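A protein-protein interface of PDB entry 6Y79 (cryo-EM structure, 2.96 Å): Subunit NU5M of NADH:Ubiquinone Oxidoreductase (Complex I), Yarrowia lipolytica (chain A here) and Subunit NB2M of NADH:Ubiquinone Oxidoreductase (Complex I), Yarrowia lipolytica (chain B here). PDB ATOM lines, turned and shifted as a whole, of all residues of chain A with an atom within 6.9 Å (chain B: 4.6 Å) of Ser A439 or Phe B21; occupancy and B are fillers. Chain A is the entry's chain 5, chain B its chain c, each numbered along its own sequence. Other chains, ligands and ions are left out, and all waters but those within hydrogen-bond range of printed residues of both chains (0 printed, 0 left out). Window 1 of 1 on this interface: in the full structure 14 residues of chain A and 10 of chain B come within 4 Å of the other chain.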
ATOM      1  N   TYR A 363      33.186  -4.678 -15.746  1.00  0.00           N
ATOM      2  CA  TYR A 363      31.741  -4.607 -15.906  1.00  0.00           C
ATOM      3  C   TYR A 363      31.293  -5.399 -17.120  1.00  0.00           C
ATOM      4  O   TYR A 363      30.467  -6.309 -17.008  1.00  0.00           O
ATOM      5  CB  TYR A 363      31.280  -3.159 -16.033  1.00  0.00           C
ATOM      6  CG  TYR A 363      31.274  -2.376 -14.744  1.00  0.00           C
ATOM      7  CD1 TYR A 363      31.505  -2.991 -13.516  1.00  0.00           C
ATOM      8  CD2 TYR A 363      31.024  -1.017 -14.754  1.00  0.00           C
ATOM      9  CE1 TYR A 363      31.495  -2.260 -12.344  1.00  0.00           C
ATOM     10  CE2 TYR A 363      31.010  -0.285 -13.595  1.00  0.00           C
ATOM     11  CZ  TYR A 363      31.245  -0.905 -12.395  1.00  0.00           C
ATOM     12  OH  TYR A 363      31.225  -0.145 -11.252  1.00  0.00           O
ATOM     13  N   GLY A 364      31.829  -5.070 -18.283  1.00  0.00           N
ATOM     14  CA  GLY A 364      31.372  -5.681 -19.509  1.00  0.00           C
ATOM     15  C   GLY A 364      30.035  -5.122 -19.927  1.00  0.00           C
ATOM     16  O   GLY A 364      29.516  -4.192 -19.342  1.00  0.00           O
ATOM     17  N   GLY A 365      29.473  -5.721 -20.973  1.00  0.00           N
ATOM     18  CA  GLY A 365      28.222  -5.230 -21.519  1.00  0.00           C
ATOM     19  C   GLY A 365      27.043  -5.588 -20.635  1.00  0.00           C
ATOM     20  O   GLY A 365      26.939  -6.700 -20.121  1.00  0.00           O
ATOM     21  N   LEU A 366      26.159  -4.609 -20.430  1.00  0.00           N
ATOM     22  CA  LEU A 366      24.964  -4.797 -19.617  1.00  0.00           C
ATOM     23  C   LEU A 366      23.760  -4.089 -20.218  1.00  0.00           C
ATOM     24  O   LEU A 366      22.813  -3.759 -19.498  1.00  0.00           O
ATOM     25  CB  LEU A 366      25.172  -4.288 -18.192  1.00  0.00           C
ATOM     26  CG  LEU A 366      26.140  -4.995 -17.253  1.00  0.00           C
ATOM     27  CD1 LEU A 366      26.324  -4.166 -16.003  1.00  0.00           C
ATOM     28  CD2 LEU A 366      25.617  -6.365 -16.909  1.00  0.00           C
ATOM     29  N   LEU A 367      23.783  -3.828 -21.524  1.00  0.00           N
ATOM     30  CA  LEU A 367      22.681  -3.116 -22.161  1.00  0.00           C
ATOM     31  C   LEU A 367      21.437  -3.984 -22.233  1.00  0.00           C
ATOM     32  O   LEU A 367      20.329  -3.530 -21.937  1.00  0.00           O
ATOM     33  CB  LEU A 367      23.092  -2.665 -23.557  1.00  0.00           C
ATOM     34  CG  LEU A 367      21.994  -1.947 -24.329  1.00  0.00           C
ATOM     35  CD1 LEU A 367      21.701  -0.685 -23.631  1.00  0.00           C
ATOM     36  CD2 LEU A 367      22.414  -1.655 -25.734  1.00  0.00           C
ATOM     37  N   SER A 368      21.618  -5.242 -22.617  1.00  0.00           N
ATOM     38  CA  SER A 368      20.538  -6.209 -22.675  1.00  0.00           C
ATOM     39  C   SER A 368      19.921  -6.474 -21.308  1.00  0.00           C
ATOM     40  O   SER A 368      18.728  -6.775 -21.225  1.00  0.00           O
ATOM     41  CB  SER A 368      21.079  -7.488 -23.273  1.00  0.00           C
ATOM     42  OG  SER A 368      22.164  -7.935 -22.488  1.00  0.00           O
ATOM     43  N   TYR A 369      20.697  -6.343 -20.235  1.00  0.00           N
ATOM     44  CA  TYR A 369      20.267  -6.788 -18.917  1.00  0.00           C
ATOM     45  C   TYR A 369      19.713  -5.658 -18.069  1.00  0.00           C
ATOM     46  O   TYR A 369      18.864  -5.898 -17.204  1.00  0.00           O
ATOM     47  CB  TYR A 369      21.440  -7.447 -18.188  1.00  0.00           C
ATOM     48  CG  TYR A 369      21.941  -8.732 -18.818  1.00  0.00           C
ATOM     49  CD1 TYR A 369      21.165  -9.444 -19.706  1.00  0.00           C
ATOM     50  CD2 TYR A 369      23.199  -9.218 -18.542  1.00  0.00           C
ATOM     51  CE1 TYR A 369      21.607 -10.612 -20.286  1.00  0.00           C
ATOM     52  CE2 TYR A 369      23.645 -10.385 -19.126  1.00  0.00           C
ATOM     53  CZ  TYR A 369      22.851 -11.077 -19.992  1.00  0.00           C
ATOM     54  OH  TYR A 369      23.309 -12.239 -20.568  1.00  0.00           O
ATOM     55  N   LEU A 433      29.917   4.963 -20.516  1.00  0.00           N
ATOM     56  CA  LEU A 433      28.774   4.338 -21.153  1.00  0.00           C
ATOM     57  C   LEU A 433      29.178   3.174 -22.034  1.00  0.00           C
ATOM     58  O   LEU A 433      28.366   2.271 -22.257  1.00  0.00           O
ATOM     59  CB  LEU A 433      27.991   5.358 -21.982  1.00  0.00           C
ATOM     60  CG  LEU A 433      26.534   4.992 -22.245  1.00  0.00           C
ATOM     61  CD1 LEU A 433      25.820   4.797 -20.942  1.00  0.00           C
ATOM     62  CD2 LEU A 433      25.857   6.068 -23.045  1.00  0.00           C
ATOM     63  N   TYR A 434      30.422   3.144 -22.514  1.00  0.00           N
ATOM     64  CA  TYR A 434      30.794   2.078 -23.437  1.00  0.00           C
ATOM     65  C   TYR A 434      31.134   0.802 -22.690  1.00  0.00           C
ATOM     66  O   TYR A 434      30.493  -0.235 -22.888  1.00  0.00           O
ATOM     67  CB  TYR A 434      31.972   2.493 -24.315  1.00  0.00           C
ATOM     68  CG  TYR A 434      32.410   1.379 -25.216  1.00  0.00           C
ATOM     69  CD1 TYR A 434      31.638   1.016 -26.301  1.00  0.00           C
ATOM     70  CD2 TYR A 434      33.579   0.671 -24.965  1.00  0.00           C
ATOM     71  CE1 TYR A 434      32.011  -0.014 -27.117  1.00  0.00           C
ATOM     72  CE2 TYR A 434      33.960  -0.360 -25.773  1.00  0.00           C
ATOM     73  CZ  TYR A 434      33.172  -0.694 -26.848  1.00  0.00           C
ATOM     74  OH  TYR A 434      33.551  -1.725 -27.655  1.00  0.00           O
ATOM     75  N   LEU A 435      32.129   0.866 -21.800  1.00  0.00           N
ATOM     76  CA  LEU A 435      32.662  -0.295 -21.090  1.00  0.00           C
ATOM     77  C   LEU A 435      31.687  -0.891 -20.091  1.00  0.00           C
ATOM     78  O   LEU A 435      31.993  -1.922 -19.481  1.00  0.00           O
ATOM     79  CB  LEU A 435      33.965   0.086 -20.386  1.00  0.00           C
ATOM     80  CG  LEU A 435      35.141   0.473 -21.292  1.00  0.00           C
ATOM     81  CD1 LEU A 435      36.298   0.993 -20.475  1.00  0.00           C
ATOM     82  CD2 LEU A 435      35.581  -0.703 -22.135  1.00  0.00           C
ATOM     83  N   THR A 436      30.530  -0.280 -19.928  1.00  0.00           N
ATOM     84  CA  THR A 436      29.557  -0.717 -18.969  1.00  0.00           C
ATOM     85  C   THR A 436      28.320  -1.270 -19.676  1.00  0.00           C
ATOM     86  O   THR A 436      27.665  -2.166 -19.154  1.00  0.00           O
ATOM     87  CB  THR A 436      29.242   0.477 -18.064  1.00  0.00           C
ATOM     88  OG1 THR A 436      30.449   0.905 -17.453  1.00  0.00           O
ATOM     89  CG2 THR A 436      28.244   0.119 -16.994  1.00  0.00           C
ATOM     90  N   PHE A 437      28.032  -0.840 -20.895  1.00  0.00           N
ATOM     91  CA  PHE A 437      26.828  -1.334 -21.552  1.00  0.00           C
ATOM     92  C   PHE A 437      27.077  -1.945 -22.922  1.00  0.00           C
ATOM     93  O   PHE A 437      26.418  -2.919 -23.274  1.00  0.00           O
ATOM     94  CB  PHE A 437      25.819  -0.187 -21.650  1.00  0.00           C
ATOM     95  CG  PHE A 437      25.278   0.240 -20.318  1.00  0.00           C
ATOM     96  CD1 PHE A 437      24.265  -0.480 -19.712  1.00  0.00           C
ATOM     97  CD2 PHE A 437      25.781   1.353 -19.666  1.00  0.00           C
ATOM     98  CE1 PHE A 437      23.764  -0.100 -18.487  1.00  0.00           C
ATOM     99  CE2 PHE A 437      25.281   1.737 -18.440  1.00  0.00           C
ATOM    100  CZ  PHE A 437      24.270   1.010 -17.850  1.00  0.00           C
ATOM    101  N   TYR A 438      28.013  -1.407 -23.696  1.00  0.00           N
ATOM    102  CA  TYR A 438      28.180  -1.799 -25.092  1.00  0.00           C
ATOM    103  C   TYR A 438      29.289  -2.811 -25.316  1.00  0.00           C
ATOM    104  O   TYR A 438      29.325  -3.447 -26.373  1.00  0.00           O
ATOM    105  CB  TYR A 438      28.493  -0.579 -25.953  1.00  0.00           C
ATOM    106  CG  TYR A 438      27.423   0.470 -26.017  1.00  0.00           C
ATOM    107  CD1 TYR A 438      26.089   0.159 -25.796  1.00  0.00           C
ATOM    108  CD2 TYR A 438      27.754   1.782 -26.315  1.00  0.00           C
ATOM    109  CE1 TYR A 438      25.121   1.129 -25.868  1.00  0.00           C
ATOM    110  CE2 TYR A 438      26.799   2.753 -26.388  1.00  0.00           C
ATOM    111  CZ  TYR A 438      25.488   2.424 -26.164  1.00  0.00           C
ATOM    112  OH  TYR A 438      24.543   3.410 -26.245  1.00  0.00           O
ATOM    113  N   SER A 439      30.208  -2.945 -24.370  1.00  0.00           N
ATOM    114  CA  SER A 439      31.413  -3.724 -24.580  1.00  0.00           C
ATOM    115  C   SER A 439      31.103  -5.218 -24.583  1.00  0.00           C
ATOM    116  O   SER A 439      30.015  -5.663 -24.215  1.00  0.00           O
ATOM    117  CB  SER A 439      32.442  -3.398 -23.501  1.00  0.00           C
ATOM    118  OG  SER A 439      33.598  -4.196 -23.637  1.00  0.00           O
ATOM    119  N   ASN A 440      32.071  -5.995 -25.049  1.00  0.00           N
ATOM    120  CA  ASN A 440      32.019  -7.427 -24.836  1.00  0.00           C
ATOM    121  C   ASN A 440      32.230  -7.702 -23.350  1.00  0.00           C
ATOM    122  O   ASN A 440      32.978  -6.973 -22.694  1.00  0.00           O
ATOM    123  CB  ASN A 440      33.083  -8.129 -25.676  1.00  0.00           C
ATOM    124  CG  ASN A 440      32.774  -8.087 -27.157  1.00  0.00           C
ATOM    125  OD1 ASN A 440      31.638  -8.316 -27.572  1.00  0.00           O
ATOM    126  ND2 ASN A 440      33.786  -7.791 -27.964  1.00  0.00           N
ATOM    127  N   PRO A 441      31.566  -8.713 -22.789  1.00  0.00           N
ATOM    128  CA  PRO A 441      31.547  -8.865 -21.332  1.00  0.00           C
ATOM    129  C   PRO A 441      32.892  -9.267 -20.754  1.00  0.00           C
ATOM    130  O   PRO A 441      33.661 -10.017 -21.355  1.00  0.00           O
ATOM    131  CB  PRO A 441      30.501  -9.962 -21.106  1.00  0.00           C
ATOM    132  CG  PRO A 441      30.417 -10.671 -22.362  1.00  0.00           C
ATOM    133  CD  PRO A 441      30.683  -9.689 -23.440  1.00  0.00           C
ATOM    134  N   ASN A 442      33.179  -8.726 -19.571  1.00  0.00           N
ATOM    135  CA  ASN A 442      34.442  -8.971 -18.898  1.00  0.00           C
ATOM    136  C   ASN A 442      34.296  -9.750 -17.606  1.00  0.00           C
ATOM    137  O   ASN A 442      35.281 -10.328 -17.140  1.00  0.00           O
ATOM    138  CB  ASN A 442      35.154  -7.646 -18.594  1.00  0.00           C
ATOM    139  CG  ASN A 442      35.561  -6.902 -19.840  1.00  0.00           C
ATOM    140  OD1 ASN A 442      36.084  -7.484 -20.779  1.00  0.00           O
ATOM    141  ND2 ASN A 442      35.322  -5.600 -19.856  1.00  0.00           N
ATOM    142  N   TYR A 448      26.187 -12.393 -14.987  1.00  0.00           N
ATOM    143  CA  TYR A 448      25.240 -12.184 -16.063  1.00  0.00           C
ATOM    144  C   TYR A 448      24.005 -13.064 -15.918  1.00  0.00           C
ATOM    145  O   TYR A 448      22.951 -12.735 -16.471  1.00  0.00           O
ATOM    146  CB  TYR A 448      25.957 -12.407 -17.390  1.00  0.00           C
ATOM    147  CG  TYR A 448      27.061 -11.397 -17.598  1.00  0.00           C
ATOM    148  CD1 TYR A 448      26.763 -10.077 -17.895  1.00  0.00           C
ATOM    149  CD2 TYR A 448      28.393 -11.749 -17.468  1.00  0.00           C
ATOM    150  CE1 TYR A 448      27.746  -9.144 -18.081  1.00  0.00           C
ATOM    151  CE2 TYR A 448      29.392 -10.814 -17.650  1.00  0.00           C
ATOM    152  CZ  TYR A 448      29.054  -9.511 -17.952  1.00  0.00           C
ATOM    153  OH  TYR A 448      30.028  -8.564 -18.139  1.00  0.00           O
ATOM    154  N   ASN A 529      36.477   2.704 -30.037  1.00  0.00           N
ATOM    155  CA  ASN A 529      36.725   1.679 -29.027  1.00  0.00           C
ATOM    156  C   ASN A 529      36.047   0.370 -29.374  1.00  0.00           C
ATOM    157  O   ASN A 529      36.456  -0.676 -28.854  1.00  0.00           O
ATOM    158  CB  ASN A 529      36.301   2.117 -27.633  1.00  0.00           C
ATOM    159  CG  ASN A 529      37.259   1.615 -26.559  1.00  0.00           C
ATOM    160  OD1 ASN A 529      37.684   0.455 -26.577  1.00  0.00           O
ATOM    161  ND2 ASN A 529      37.643   2.497 -25.656  1.00  0.00           N
ATOM    162  N   GLU A 530      35.024   0.369 -30.240  1.00  0.00           N
ATOM    163  CA  GLU A 530      34.633  -0.966 -30.679  1.00  0.00           C
ATOM    164  C   GLU A 530      35.421  -1.426 -31.905  1.00  0.00           C
ATOM    165  O   GLU A 530      36.121  -2.437 -31.814  1.00  0.00           O
ATOM    166  CB  GLU A 530      33.139  -1.124 -30.864  1.00  0.00           C
ATOM    167  CG  GLU A 530      32.758  -2.616 -30.651  1.00  0.00           C
ATOM    168  CD  GLU A 530      32.847  -3.473 -31.893  1.00  0.00           C
ATOM    169  OE1 GLU A 530      32.404  -2.976 -32.972  1.00  0.00           O
ATOM    170  OE2 GLU A 530      33.446  -4.565 -31.826  1.00  0.00           O
ATOM    171  N   ARG B  16      31.238 -14.863 -24.723  1.00  0.00           N
ATOM    172  CA  ARG B  16      31.319 -13.412 -24.761  1.00  0.00           C
ATOM    173  C   ARG B  16      31.033 -12.851 -26.145  1.00  0.00           C
ATOM    174  O   ARG B  16      30.815 -11.645 -26.278  1.00  0.00           O
ATOM    175  CB  ARG B  16      32.697 -12.962 -24.295  1.00  0.00           C
ATOM    176  CG  ARG B  16      33.024 -13.390 -22.896  1.00  0.00           C
ATOM    177  CD  ARG B  16      34.423 -12.989 -22.524  1.00  0.00           C
ATOM    178  NE  ARG B  16      34.600 -13.019 -21.080  1.00  0.00           N
ATOM    179  CZ  ARG B  16      35.039 -14.074 -20.408  1.00  0.00           C
ATOM    180  NH1 ARG B  16      35.164 -14.014 -19.094  1.00  0.00           N
ATOM    181  NH2 ARG B  16      35.356 -15.185 -21.055  1.00  0.00           N
ATOM    182  N   TYR B  17      31.049 -13.689 -27.176  1.00  0.00           N
ATOM    183  CA  TYR B  17      30.804 -13.252 -28.540  1.00  0.00           C
ATOM    184  C   TYR B  17      29.526 -13.825 -29.120  1.00  0.00           C
ATOM    185  O   TYR B  17      29.129 -13.433 -30.220  1.00  0.00           O
ATOM    186  CB  TYR B  17      31.993 -13.632 -29.426  1.00  0.00           C
ATOM    187  CG  TYR B  17      33.224 -12.873 -29.036  1.00  0.00           C
ATOM    188  CD1 TYR B  17      33.437 -11.593 -29.516  1.00  0.00           C
ATOM    189  CD2 TYR B  17      34.153 -13.412 -28.153  1.00  0.00           C
ATOM    190  CE1 TYR B  17      34.549 -10.877 -29.154  1.00  0.00           C
ATOM    191  CE2 TYR B  17      35.271 -12.701 -27.780  1.00  0.00           C
ATOM    192  CZ  TYR B  17      35.461 -11.433 -28.288  1.00  0.00           C
ATOM    193  OH  TYR B  17      36.558 -10.696 -27.935  1.00  0.00           O
ATOM    194  N   GLN B  18      28.881 -14.731 -28.407  1.00  0.00           N
ATOM    195  CA  GLN B  18      27.679 -15.411 -28.855  1.00  0.00           C
ATOM    196  C   GLN B  18      26.451 -14.636 -28.372  1.00  0.00           C
ATOM    197  O   GLN B  18      26.541 -13.453 -28.036  1.00  0.00           O
ATOM    198  CB  GLN B  18      27.728 -16.878 -28.420  1.00  0.00           C
ATOM    199  CG  GLN B  18      28.657 -17.695 -29.309  1.00  0.00           C
ATOM    200  CD  GLN B  18      28.997 -19.057 -28.750  1.00  0.00           C
ATOM    201  OE1 GLN B  18      28.463 -19.471 -27.726  1.00  0.00           O
ATOM    202  NE2 GLN B  18      29.903 -19.760 -29.421  1.00  0.00           N
ATOM    203  N   THR B  19      25.311 -15.322 -28.314  1.00  0.00           N
ATOM    204  CA  THR B  19      23.935 -14.862 -28.501  1.00  0.00           C
ATOM    205  C   THR B  19      23.513 -13.480 -27.988  1.00  0.00           C
ATOM    206  O   THR B  19      22.675 -12.835 -28.623  1.00  0.00           O
ATOM    207  CB  THR B  19      23.032 -15.929 -27.889  1.00  0.00           C
ATOM    208  OG1 THR B  19      21.665 -15.512 -27.915  1.00  0.00           O
ATOM    209  CG2 THR B  19      23.482 -16.263 -26.493  1.00  0.00           C
ATOM    210  N   ASN B  20      24.038 -13.001 -26.859  1.00  0.00           N
ATOM    211  CA  ASN B  20      23.578 -11.712 -26.343  1.00  0.00           C
ATOM    212  C   ASN B  20      24.592 -10.606 -26.539  1.00  0.00           C
ATOM    213  O   ASN B  20      24.236  -9.423 -26.491  1.00  0.00           O
ATOM    214  CB  ASN B  20      23.235 -11.823 -24.860  1.00  0.00           C
ATOM    215  CG  ASN B  20      22.096 -12.776 -24.606  1.00  0.00           C
ATOM    216  OD1 ASN B  20      21.421 -13.222 -25.534  1.00  0.00           O
ATOM    217  ND2 ASN B  20      21.865 -13.091 -23.338  1.00  0.00           N
ATOM    218  N   PHE B  21      25.846 -10.967 -26.745  1.00  0.00           N
ATOM    219  CA  PHE B  21      26.898 -10.004 -27.003  1.00  0.00           C
ATOM    220  C   PHE B  21      27.458 -10.204 -28.400  1.00  0.00           C
ATOM    221  O   PHE B  21      28.644  -9.995 -28.657  1.00  0.00           O
ATOM    222  CB  PHE B  21      27.953 -10.089 -25.911  1.00  0.00           C
ATOM    223  CG  PHE B  21      27.401  -9.772 -24.560  1.00  0.00           C
ATOM    224  CD1 PHE B  21      27.179  -8.454 -24.194  1.00  0.00           C
ATOM    225  CD2 PHE B  21      27.054 -10.781 -23.675  1.00  0.00           C
ATOM    226  CE1 PHE B  21      26.649  -8.143 -22.962  1.00  0.00           C
ATOM    227  CE2 PHE B  21      26.529 -10.477 -22.434  1.00  0.00           C
ATOM    228  CZ  PHE B  21      26.326  -9.155 -22.079  1.00  0.00           C
ATOM    229  N   THR B  22      26.576 -10.608 -29.306  1.00  0.00           N
ATOM    230  CA  THR B  22      26.806 -10.430 -30.720  1.00  0.00           C
ATOM    231  C   THR B  22      26.873  -8.952 -31.042  1.00  0.00           C
ATOM    232  O   THR B  22      26.392  -8.108 -30.288  1.00  0.00           O
ATOM    233  CB  THR B  22      25.683 -11.037 -31.524  1.00  0.00           C
ATOM    234  OG1 THR B  22      24.541 -10.186 -31.436  1.00  0.00           O
ATOM    235  CG2 THR B  22      25.325 -12.385 -30.968  1.00  0.00           C
ATOM    236  N   ARG B  23      27.448  -8.642 -32.202  1.00  0.00           N
ATOM    237  CA  ARG B  23      27.522  -7.253 -32.631  1.00  0.00           C
ATOM    238  C   ARG B  23      26.136  -6.674 -32.894  1.00  0.00           C
ATOM    239  O   ARG B  23      25.873  -5.509 -32.576  1.00  0.00           O
ATOM    240  CB  ARG B  23      28.390  -7.146 -33.869  1.00  0.00           C
ATOM    241  CG  ARG B  23      28.574  -5.734 -34.362  1.00  0.00           C
ATOM    242  CD  ARG B  23      29.433  -5.797 -35.581  1.00  0.00           C
ATOM    243  NE  ARG B  23      30.778  -6.189 -35.214  1.00  0.00           N
ATOM    244  CZ  ARG B  23      31.747  -5.379 -34.869  1.00  0.00           C
ATOM    245  NH1 ARG B  23      32.926  -5.868 -34.545  1.00  0.00           N
ATOM    246  NH2 ARG B  23      31.550  -4.099 -34.867  1.00  0.00           N
ATOM    247  N   ARG B  26      24.433  -6.010 -29.336  1.00  0.00           N
ATOM    248  CA  ARG B  26      25.080  -5.024 -28.473  1.00  0.00           C
ATOM    249  C   ARG B  26      24.594  -3.610 -28.762  1.00  0.00           C
ATOM    250  O   ARG B  26      24.607  -2.761 -27.868  1.00  0.00           O
ATOM    251  CB  ARG B  26      26.603  -5.094 -28.617  1.00  0.00           C
ATOM    252  CG  ARG B  26      27.296  -6.198 -27.818  1.00  0.00           C
ATOM    253  CD  ARG B  26      28.802  -6.190 -28.077  1.00  0.00           C
ATOM    254  NE  ARG B  26      29.105  -6.171 -29.505  1.00  0.00           N
ATOM    255  CZ  ARG B  26      30.332  -6.096 -30.005  1.00  0.00           C
ATOM    256  NH1 ARG B  26      30.522  -6.078 -31.319  1.00  0.00           N
ATOM    257  NH2 ARG B  26      31.369  -6.037 -29.188  1.00  0.00           N
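The guanidinium group (NH1) of Arg B23 lies within salt-bridge range of the side-chain carboxylate (OE2) of Glu A530 (3.1 Å). The guanidinium group (NH1) of Arg B26 is in salt-bridge range of the side-chain carboxylate (OE2) of Glu A530 (3.3 Å). NH2 of Arg B26 lies within hydrogen-bond range of OD1 of Asn A440, 2.8 Å away. The side-chain amide nitrogen of Asn B20 is in hydrogen-bond range of the side-chain hydroxyl of Tyr A369 (3.2 Å). The backbone carbonyl oxygen (O) of Pro A441 lies within hydrogen-bond range of the guanidinium group (NE) of Arg B16 (3.2 Å).
The side-chain hydroxyl of Thr B19 sits close to the side-chain amide oxygen of Asn B20 (3.3 Å). The backbone NH (N) of Leu A367 lies within hydrogen-bond range of the backbone carbonyl oxygen (O) of Phe A437 (3.3 Å). The guanidinium group (NE) of Arg B26 lies close to the backbone carbonyl oxygen (O) of Thr B22 (3.4 Å). The backbone NH (N) of Gly A365 sits close to the backbone carbonyl oxygen (O) of Ser A439. The backbone NH (N) of Ser A439 sits at hydrogen-bond distance from the backbone carbonyl oxygen (O) of Tyr A434 (3.1 Å).
Gly A365 touches Phe B21 (O to CZ, 3.2 Å). CD2 of Leu A367 touches O of Arg B26 (3.3 Å). Tyr A438 touches Arg B26. Ser A439 touches Phe B21. O of Arg B16 touches OD1 of Asn A440, 3.7 Å away. Asn A440 touches Tyr B17 (ND2 to CE1, 3.4 Å). OD1 of Asn A440 touches O of Phe B21, 3.6 Å away. CG of Phe B21 touches CD of Pro A441 (3.5 Å).
Of chain B, only Phe B21 (3.98 Å) comes within 4 Å of Ser A439. Of chain A, only Gly A365 (3.2 Å), Ser A439 (3.98 Å), Asn A440 (3.6 Å) and Pro A441 (3.5 Å) come within 4 Å of Phe B21. Of the printed residues of chain B, Leu A367 touches Arg B26. Of the printed residues of chain B, Pro A441 touches Arg B16 and Phe B21. Leu A433 touches none of the printed residues of chain B. Thr B22 touches none of the printed residues of chain A. The nearest residue of chain B that does not touch Ser A439 is Arg B26 (4.1 Å). The nearest residue of chain A that does not touch Phe B21 is Tyr A369 (4.1 Å).
Of the 20 printed residues of chain A, 8 touch a printed residue of chain B. Hydrophobic or aromatic side chains of chain A that line the printed part of chain B: Leu A367, Tyr A369, Tyr A438 and Pro A441. Of the 9 printed residues of chain B, 6 touch a printed residue of chain A. Hydrophobic or aromatic side chains of chain B that line the printed part of chain A: Tyr B17 and Phe B21. Among the printed residues, 13 pairs touch across the chains. Among the printed residues, Asp or Glu carboxylates within 4 Å of a Lys or Arg side-chain nitrogen of the other chain: Glu A530 with Arg B23 (2.4 Å) and Glu A530 with Arg B26 (3.3 Å).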
